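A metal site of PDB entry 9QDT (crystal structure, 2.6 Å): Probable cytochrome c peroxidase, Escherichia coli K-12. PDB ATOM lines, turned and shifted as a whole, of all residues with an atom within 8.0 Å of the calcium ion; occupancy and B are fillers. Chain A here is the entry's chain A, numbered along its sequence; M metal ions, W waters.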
ATOM      1  N   VAL A 173     -20.560  35.363 -28.618  1.00  0.00           N
ATOM      2  CA  VAL A 173     -19.701  34.193 -28.610  1.00  0.00           C
ATOM      3  C   VAL A 173     -19.044  34.036 -29.988  1.00  0.00           C
ATOM      4  O   VAL A 173     -19.497  34.655 -30.956  1.00  0.00           O
ATOM      5  CB  VAL A 173     -20.804  33.183 -28.241  1.00  0.00           C
ATOM      6  CG1 VAL A 173     -20.905  32.028 -29.201  1.00  0.00           C
ATOM      7  CG2 VAL A 173     -20.757  32.764 -26.772  1.00  0.00           C
ATOM      8  N   ASP A 174     -17.966  33.227 -30.084  1.00  0.00           N
ATOM      9  CA  ASP A 174     -17.228  33.088 -31.331  1.00  0.00           C
ATOM     10  C   ASP A 174     -17.702  31.892 -32.160  1.00  0.00           C
ATOM     11  O   ASP A 174     -17.293  31.755 -33.324  1.00  0.00           O
ATOM     12  CB  ASP A 174     -15.741  32.998 -31.075  1.00  0.00           C
ATOM     13  CG  ASP A 174     -15.291  31.937 -30.084  1.00  0.00           C
ATOM     14  OD1 ASP A 174     -16.134  31.041 -29.727  1.00  0.00           O
ATOM     15  OD2 ASP A 174     -14.104  32.024 -29.657  1.00  0.00           O
ATOM     16  N   GLY A 175     -18.509  31.008 -31.554  1.00  0.00           N
ATOM     17  CA  GLY A 175     -19.069  29.851 -32.227  1.00  0.00           C
ATOM     18  C   GLY A 175     -18.042  28.738 -32.475  1.00  0.00           C
ATOM     19  O   GLY A 175     -18.304  27.774 -33.176  1.00  0.00           O
ATOM     20  N   ARG A 176     -16.855  28.901 -31.894  1.00  0.00           N
ATOM     21  CA  ARG A 176     -15.810  27.907 -31.955  1.00  0.00           C
ATOM     22  C   ARG A 176     -15.871  27.001 -30.720  1.00  0.00           C
ATOM     23  O   ARG A 176     -16.440  27.354 -29.684  1.00  0.00           O
ATOM     24  CB  ARG A 176     -14.452  28.601 -31.942  1.00  0.00           C
ATOM     25  CG  ARG A 176     -14.236  29.737 -32.917  1.00  0.00           C
ATOM     26  CD  ARG A 176     -12.801  30.278 -32.819  1.00  0.00           C
ATOM     27  NE  ARG A 176     -12.600  31.452 -33.685  1.00  0.00           N
ATOM     28  CZ  ARG A 176     -12.182  31.370 -34.923  1.00  0.00           C
ATOM     29  NH1 ARG A 176     -11.824  30.206 -35.438  1.00  0.00           N
ATOM     30  NH2 ARG A 176     -12.106  32.463 -35.635  1.00  0.00           N
ATOM     31  N   LYS A 177     -15.232  25.831 -30.858  1.00  0.00           N
ATOM     32  CA  LYS A 177     -15.109  24.846 -29.803  1.00  0.00           C
ATOM     33  C   LYS A 177     -14.414  25.471 -28.588  1.00  0.00           C
ATOM     34  O   LYS A 177     -14.908  25.400 -27.476  1.00  0.00           O
ATOM     35  CB  LYS A 177     -14.320  23.698 -30.429  1.00  0.00           C
ATOM     36  CG  LYS A 177     -14.231  22.516 -29.538  1.00  0.00           C
ATOM     37  CD  LYS A 177     -13.353  21.393 -30.053  1.00  0.00           C
ATOM     38  CE  LYS A 177     -13.531  20.244 -29.123  1.00  0.00           C
ATOM     39  NZ  LYS A 177     -12.409  19.311 -29.198  1.00  0.00           N
ATOM     40  N   ASN A 190     -14.608  26.555 -23.817  1.00  0.00           N
ATOM     41  CA  ASN A 190     -15.573  27.231 -24.666  1.00  0.00           C
ATOM     42  C   ASN A 190     -15.872  28.592 -24.068  1.00  0.00           C
ATOM     43  O   ASN A 190     -16.093  28.690 -22.876  1.00  0.00           O
ATOM     44  CB  ASN A 190     -16.869  26.410 -24.769  1.00  0.00           C
ATOM     45  CG  ASN A 190     -17.873  26.939 -25.766  1.00  0.00           C
ATOM     46  OD1 ASN A 190     -18.959  27.448 -25.407  1.00  0.00           O
ATOM     47  ND2 ASN A 190     -17.570  26.804 -27.044  1.00  0.00           N
ATOM     48  N   ALA A 191     -15.929  29.608 -24.918  1.00  0.00           N
ATOM     49  CA  ALA A 191     -16.170  30.975 -24.477  1.00  0.00           C
ATOM     50  C   ALA A 191     -17.658  31.128 -24.269  1.00  0.00           C
ATOM     51  O   ALA A 191     -18.434  30.918 -25.180  1.00  0.00           O
ATOM     52  CB  ALA A 191     -15.672  31.957 -25.515  1.00  0.00           C
ATOM     53  N   PRO A 192     -18.097  31.526 -23.057  1.00  0.00           N
ATOM     54  CA  PRO A 192     -19.512  31.746 -22.818  1.00  0.00           C
ATOM     55  C   PRO A 192     -19.920  33.115 -23.329  1.00  0.00           C
ATOM     56  O   PRO A 192     -19.066  33.945 -23.634  1.00  0.00           O
ATOM     57  CB  PRO A 192     -19.613  31.644 -21.305  1.00  0.00           C
ATOM     58  CG  PRO A 192     -18.273  32.163 -20.827  1.00  0.00           C
ATOM     59  CD  PRO A 192     -17.268  31.720 -21.872  1.00  0.00           C
ATOM     60  N   THR A 193     -21.242  33.314 -23.403  1.00  0.00           N
ATOM     61  CA  THR A 193     -21.841  34.558 -23.828  1.00  0.00           C
ATOM     62  C   THR A 193     -21.629  35.662 -22.794  1.00  0.00           C
ATOM     63  O   THR A 193     -21.683  35.455 -21.582  1.00  0.00           O
ATOM     64  CB  THR A 193     -23.324  34.312 -24.118  1.00  0.00           C
ATOM     65  OG1 THR A 193     -23.755  35.527 -24.727  1.00  0.00           O
ATOM     66  CG2 THR A 193     -24.092  33.972 -22.851  1.00  0.00           C
ATOM     67  N   TRP A 205     -15.949  29.839 -15.982  1.00  0.00           N
ATOM     68  CA  TRP A 205     -16.520  28.534 -15.679  1.00  0.00           C
ATOM     69  C   TRP A 205     -16.153  28.128 -14.252  1.00  0.00           C
ATOM     70  O   TRP A 205     -16.988  27.560 -13.553  1.00  0.00           O
ATOM     71  CB  TRP A 205     -16.032  27.495 -16.697  1.00  0.00           C
ATOM     72  CG  TRP A 205     -16.699  27.536 -18.040  1.00  0.00           C
ATOM     73  CD1 TRP A 205     -16.239  28.134 -19.187  1.00  0.00           C
ATOM     74  CD2 TRP A 205     -17.932  26.889 -18.401  1.00  0.00           C
ATOM     75  NE1 TRP A 205     -17.112  27.916 -20.216  1.00  0.00           N
ATOM     76  CE2 TRP A 205     -18.164  27.158 -19.765  1.00  0.00           C
ATOM     77  CE3 TRP A 205     -18.870  26.121 -17.693  1.00  0.00           C
ATOM     78  CZ2 TRP A 205     -19.276  26.674 -20.442  1.00  0.00           C
ATOM     79  CZ3 TRP A 205     -19.962  25.624 -18.366  1.00  0.00           C
ATOM     80  CH2 TRP A 205     -20.163  25.898 -19.720  1.00  0.00           C
ATOM     81  N   PRO A 357     -24.322  26.968 -16.542  1.00  0.00           N
ATOM     82  CA  PRO A 357     -24.562  27.989 -17.561  1.00  0.00           C
ATOM     83  C   PRO A 357     -26.005  28.447 -17.530  1.00  0.00           C
ATOM     84  O   PRO A 357     -26.912  27.613 -17.436  1.00  0.00           O
ATOM     85  CB  PRO A 357     -24.241  27.287 -18.887  1.00  0.00           C
ATOM     86  CG  PRO A 357     -23.650  25.967 -18.497  1.00  0.00           C
ATOM     87  CD  PRO A 357     -24.114  25.628 -17.109  1.00  0.00           C
ATOM     88  N   VAL A 362     -29.351  30.231 -25.335  1.00  0.00           N
ATOM     89  CA  VAL A 362     -28.521  29.054 -25.569  1.00  0.00           C
ATOM     90  C   VAL A 362     -28.675  28.580 -27.016  1.00  0.00           C
ATOM     91  O   VAL A 362     -27.762  27.974 -27.576  1.00  0.00           O
ATOM     92  CB  VAL A 362     -28.842  27.910 -24.594  1.00  0.00           C
ATOM     93  CG1 VAL A 362     -30.249  27.377 -24.785  1.00  0.00           C
ATOM     94  CG2 VAL A 362     -27.813  26.787 -24.728  1.00  0.00           C
ATOM     95  N   LEU A 364     -28.408  30.246 -29.452  1.00  0.00           N
ATOM     96  CA  LEU A 364     -27.535  31.056 -30.274  1.00  0.00           C
ATOM     97  C   LEU A 364     -26.053  30.864 -29.923  1.00  0.00           C
ATOM     98  O   LEU A 364     -25.230  31.544 -30.531  1.00  0.00           O
ATOM     99  CB  LEU A 364     -27.843  32.536 -30.080  1.00  0.00           C
ATOM    100  CG  LEU A 364     -29.283  32.996 -30.331  1.00  0.00           C
ATOM    101  CD1 LEU A 364     -29.318  34.497 -30.053  1.00  0.00           C
ATOM    102  CD2 LEU A 364     -29.759  32.636 -31.739  1.00  0.00           C
ATOM    103  N   THR A 365     -25.731  30.035 -28.915  1.00  0.00           N
ATOM    104  CA  THR A 365     -24.360  29.948 -28.420  1.00  0.00           C
ATOM    105  C   THR A 365     -23.742  28.546 -28.622  1.00  0.00           C
ATOM    106  O   THR A 365     -22.799  28.198 -27.912  1.00  0.00           O
ATOM    107  CB  THR A 365     -24.396  30.384 -26.958  1.00  0.00           C
ATOM    108  OG1 THR A 365     -25.233  29.510 -26.189  1.00  0.00           O
ATOM    109  CG2 THR A 365     -25.000  31.768 -26.844  1.00  0.00           C
ATOM    110  N   ALA A 366     -24.237  27.765 -29.600  1.00  0.00           N
ATOM    111  CA  ALA A 366     -23.511  26.575 -30.043  1.00  0.00           C
ATOM    112  C   ALA A 366     -22.029  26.855 -30.316  1.00  0.00           C
ATOM    113  O   ALA A 366     -21.623  27.974 -30.593  1.00  0.00           O
ATOM    114  CB  ALA A 366     -24.160  26.006 -31.281  1.00  0.00           C
ATOM    115  N   PRO A 367     -21.117  25.866 -30.177  1.00  0.00           N
ATOM    116  CA  PRO A 367     -21.423  24.560 -29.583  1.00  0.00           C
ATOM    117  C   PRO A 367     -21.476  24.612 -28.052  1.00  0.00           C
ATOM    118  O   PRO A 367     -21.138  25.653 -27.465  1.00  0.00           O
ATOM    119  CB  PRO A 367     -20.250  23.707 -30.076  1.00  0.00           C
ATOM    120  CG  PRO A 367     -19.086  24.674 -30.134  1.00  0.00           C
ATOM    121  CD  PRO A 367     -19.713  25.988 -30.587  1.00  0.00           C
ATOM    122  N   TYR A 368     -21.857  23.471 -27.432  1.00  0.00           N
ATOM    123  CA  TYR A 368     -22.246  23.449 -26.025  1.00  0.00           C
ATOM    124  C   TYR A 368     -21.262  22.692 -25.140  1.00  0.00           C
ATOM    125  O   TYR A 368     -20.367  22.004 -25.630  1.00  0.00           O
ATOM    126  CB  TYR A 368     -23.653  22.843 -25.971  1.00  0.00           C
ATOM    127  CG  TYR A 368     -24.605  23.654 -26.814  1.00  0.00           C
ATOM    128  CD1 TYR A 368     -24.947  24.935 -26.424  1.00  0.00           C
ATOM    129  CD2 TYR A 368     -25.124  23.170 -28.003  1.00  0.00           C
ATOM    130  CE1 TYR A 368     -25.762  25.725 -27.202  1.00  0.00           C
ATOM    131  CE2 TYR A 368     -25.948  23.949 -28.799  1.00  0.00           C
ATOM    132  CZ  TYR A 368     -26.258  25.236 -28.399  1.00  0.00           C
ATOM    133  OH  TYR A 368     -27.103  26.008 -29.135  1.00  0.00           O
ATOM    134  N   PHE A 369     -21.489  22.817 -23.819  1.00  0.00           N
ATOM    135  CA  PHE A 369     -20.669  22.280 -22.743  1.00  0.00           C
ATOM    136  C   PHE A 369     -19.332  23.008 -22.712  1.00  0.00           C
ATOM    137  O   PHE A 369     -18.960  23.729 -23.639  1.00  0.00           O
ATOM    138  CB  PHE A 369     -20.519  20.749 -22.786  1.00  0.00           C
ATOM    139  CG  PHE A 369     -21.748  19.935 -22.406  1.00  0.00           C
ATOM    140  CD1 PHE A 369     -23.034  20.435 -22.514  1.00  0.00           C
ATOM    141  CD2 PHE A 369     -21.611  18.668 -21.880  1.00  0.00           C
ATOM    142  CE1 PHE A 369     -24.138  19.682 -22.137  1.00  0.00           C
ATOM    143  CE2 PHE A 369     -22.722  17.910 -21.509  1.00  0.00           C
ATOM    144  CZ  PHE A 369     -23.981  18.420 -21.647  1.00  0.00           C
ATOM    145  N   HIS A 370     -18.630  22.889 -21.595  1.00  0.00           N
ATOM    146  CA  HIS A 370     -17.419  23.667 -21.401  1.00  0.00           C
ATOM    147  C   HIS A 370     -16.326  23.239 -22.384  1.00  0.00           C
ATOM    148  O   HIS A 370     -15.419  24.024 -22.682  1.00  0.00           O
ATOM    149  CB  HIS A 370     -16.991  23.637 -19.934  1.00  0.00           C
ATOM    150  CG  HIS A 370     -16.275  22.403 -19.488  1.00  0.00           C
ATOM    151  ND1 HIS A 370     -16.838  21.482 -18.627  1.00  0.00           N
ATOM    152  CD2 HIS A 370     -15.040  21.984 -19.749  1.00  0.00           C
ATOM    153  CE1 HIS A 370     -15.950  20.521 -18.397  1.00  0.00           C
ATOM    154  NE2 HIS A 370     -14.846  20.800 -19.080  1.00  0.00           N
ATOM    155  N   ARG A 371     -16.390  22.004 -22.874  1.00  0.00           N
ATOM    156  CA  ARG A 371     -15.407  21.440 -23.798  1.00  0.00           C
ATOM    157  C   ARG A 371     -15.693  21.905 -25.222  1.00  0.00           C
ATOM    158  O   ARG A 371     -14.850  21.750 -26.107  1.00  0.00           O
ATOM    159  CB  ARG A 371     -15.414  19.895 -23.691  1.00  0.00           C
ATOM    160  CG  ARG A 371     -14.240  19.408 -22.874  1.00  0.00           C
ATOM    161  CD  ARG A 371     -14.407  18.348 -21.822  1.00  0.00           C
ATOM    162  NE  ARG A 371     -14.196  17.000 -22.299  1.00  0.00           N
ATOM    163  CZ  ARG A 371     -13.354  16.052 -21.905  1.00  0.00           C
ATOM    164  NH1 ARG A 371     -12.493  16.135 -20.907  1.00  0.00           N
ATOM    165  NH2 ARG A 371     -13.432  14.930 -22.555  1.00  0.00           N
ATOM    166  N   GLY A 372     -16.911  22.385 -25.476  1.00  0.00           N
ATOM    167  CA  GLY A 372     -17.294  22.938 -26.758  1.00  0.00           C
ATOM    168  C   GLY A 372     -17.515  21.844 -27.787  1.00  0.00           C
ATOM    169  O   GLY A 372     -17.474  22.113 -29.002  1.00  0.00           O
ATOM    170  N   ASP A 373     -17.780  20.638 -27.299  1.00  0.00           N
ATOM    171  CA  ASP A 373     -17.757  19.440 -28.152  1.00  0.00           C
ATOM    172  C   ASP A 373     -19.162  18.895 -28.376  1.00  0.00           C
ATOM    173  O   ASP A 373     -19.322  17.826 -28.955  1.00  0.00           O
ATOM    174  CB  ASP A 373     -16.857  18.364 -27.565  1.00  0.00           C
ATOM    175  CG  ASP A 373     -17.231  17.826 -26.189  1.00  0.00           C
ATOM    176  OD1 ASP A 373     -18.117  18.450 -25.499  1.00  0.00           O
ATOM    177  OD2 ASP A 373     -16.632  16.775 -25.799  1.00  0.00           O
ATOM    178  N   VAL A 374     -20.198  19.592 -27.890  1.00  0.00           N
ATOM    179  CA  VAL A 374     -21.559  19.097 -28.064  1.00  0.00           C
ATOM    180  C   VAL A 374     -22.238  20.001 -29.067  1.00  0.00           C
ATOM    181  O   VAL A 374     -22.580  21.126 -28.746  1.00  0.00           O
ATOM    182  CB  VAL A 374     -22.337  19.049 -26.751  1.00  0.00           C
ATOM    183  CG1 VAL A 374     -23.801  18.658 -26.961  1.00  0.00           C
ATOM    184  CG2 VAL A 374     -21.648  18.135 -25.753  1.00  0.00           C
HETATM  185 CA    CA M   1     -21.262  27.535 -26.031  1.00  0.00          CA
HETATM  186  O   HOH W   1     -20.168  28.284 -28.124  1.00  0.00           O
HETATM  187  O   HOH W   2     -20.880  29.865 -25.593  1.00  0.00           O
HETATM  188  O   HOH W   3     -20.944  25.963 -24.236  1.00  0.00           O
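The calcium ion is bound by O of Pro 367, OD1 of Asn 190, water W2, water W3, water W1 and O of Thr 365.
The calcium ion has six donor atoms within binding distance.
ND2 of Asn 190 sits at hydrogen-bond distance from O of Lys 177, at 3.0 Å.
ND2 of Asn 190 is in hydrogen-bond range of O of Arg 176 (2.9 Å).
NE1 of Trp 205 is in hydrogen-bond range of O of Asn 190 (3.0 Å).
N of Asn 190 sits at hydrogen-bond distance from O of His 370 (2.9 Å).
The side-chain hydroxyl of Thr 365 lies within hydrogen-bond range of the backbone carbonyl oxygen of Val 362, 3.3 Å away.
Three residues have an atom within 4 Å of the calcium ion: Asn 190, Thr 365 and Pro 367.
Water W1 bridges the backbone carbonyl oxygen of Ala 366 and the side-chain amide nitrogen of Asn 190.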
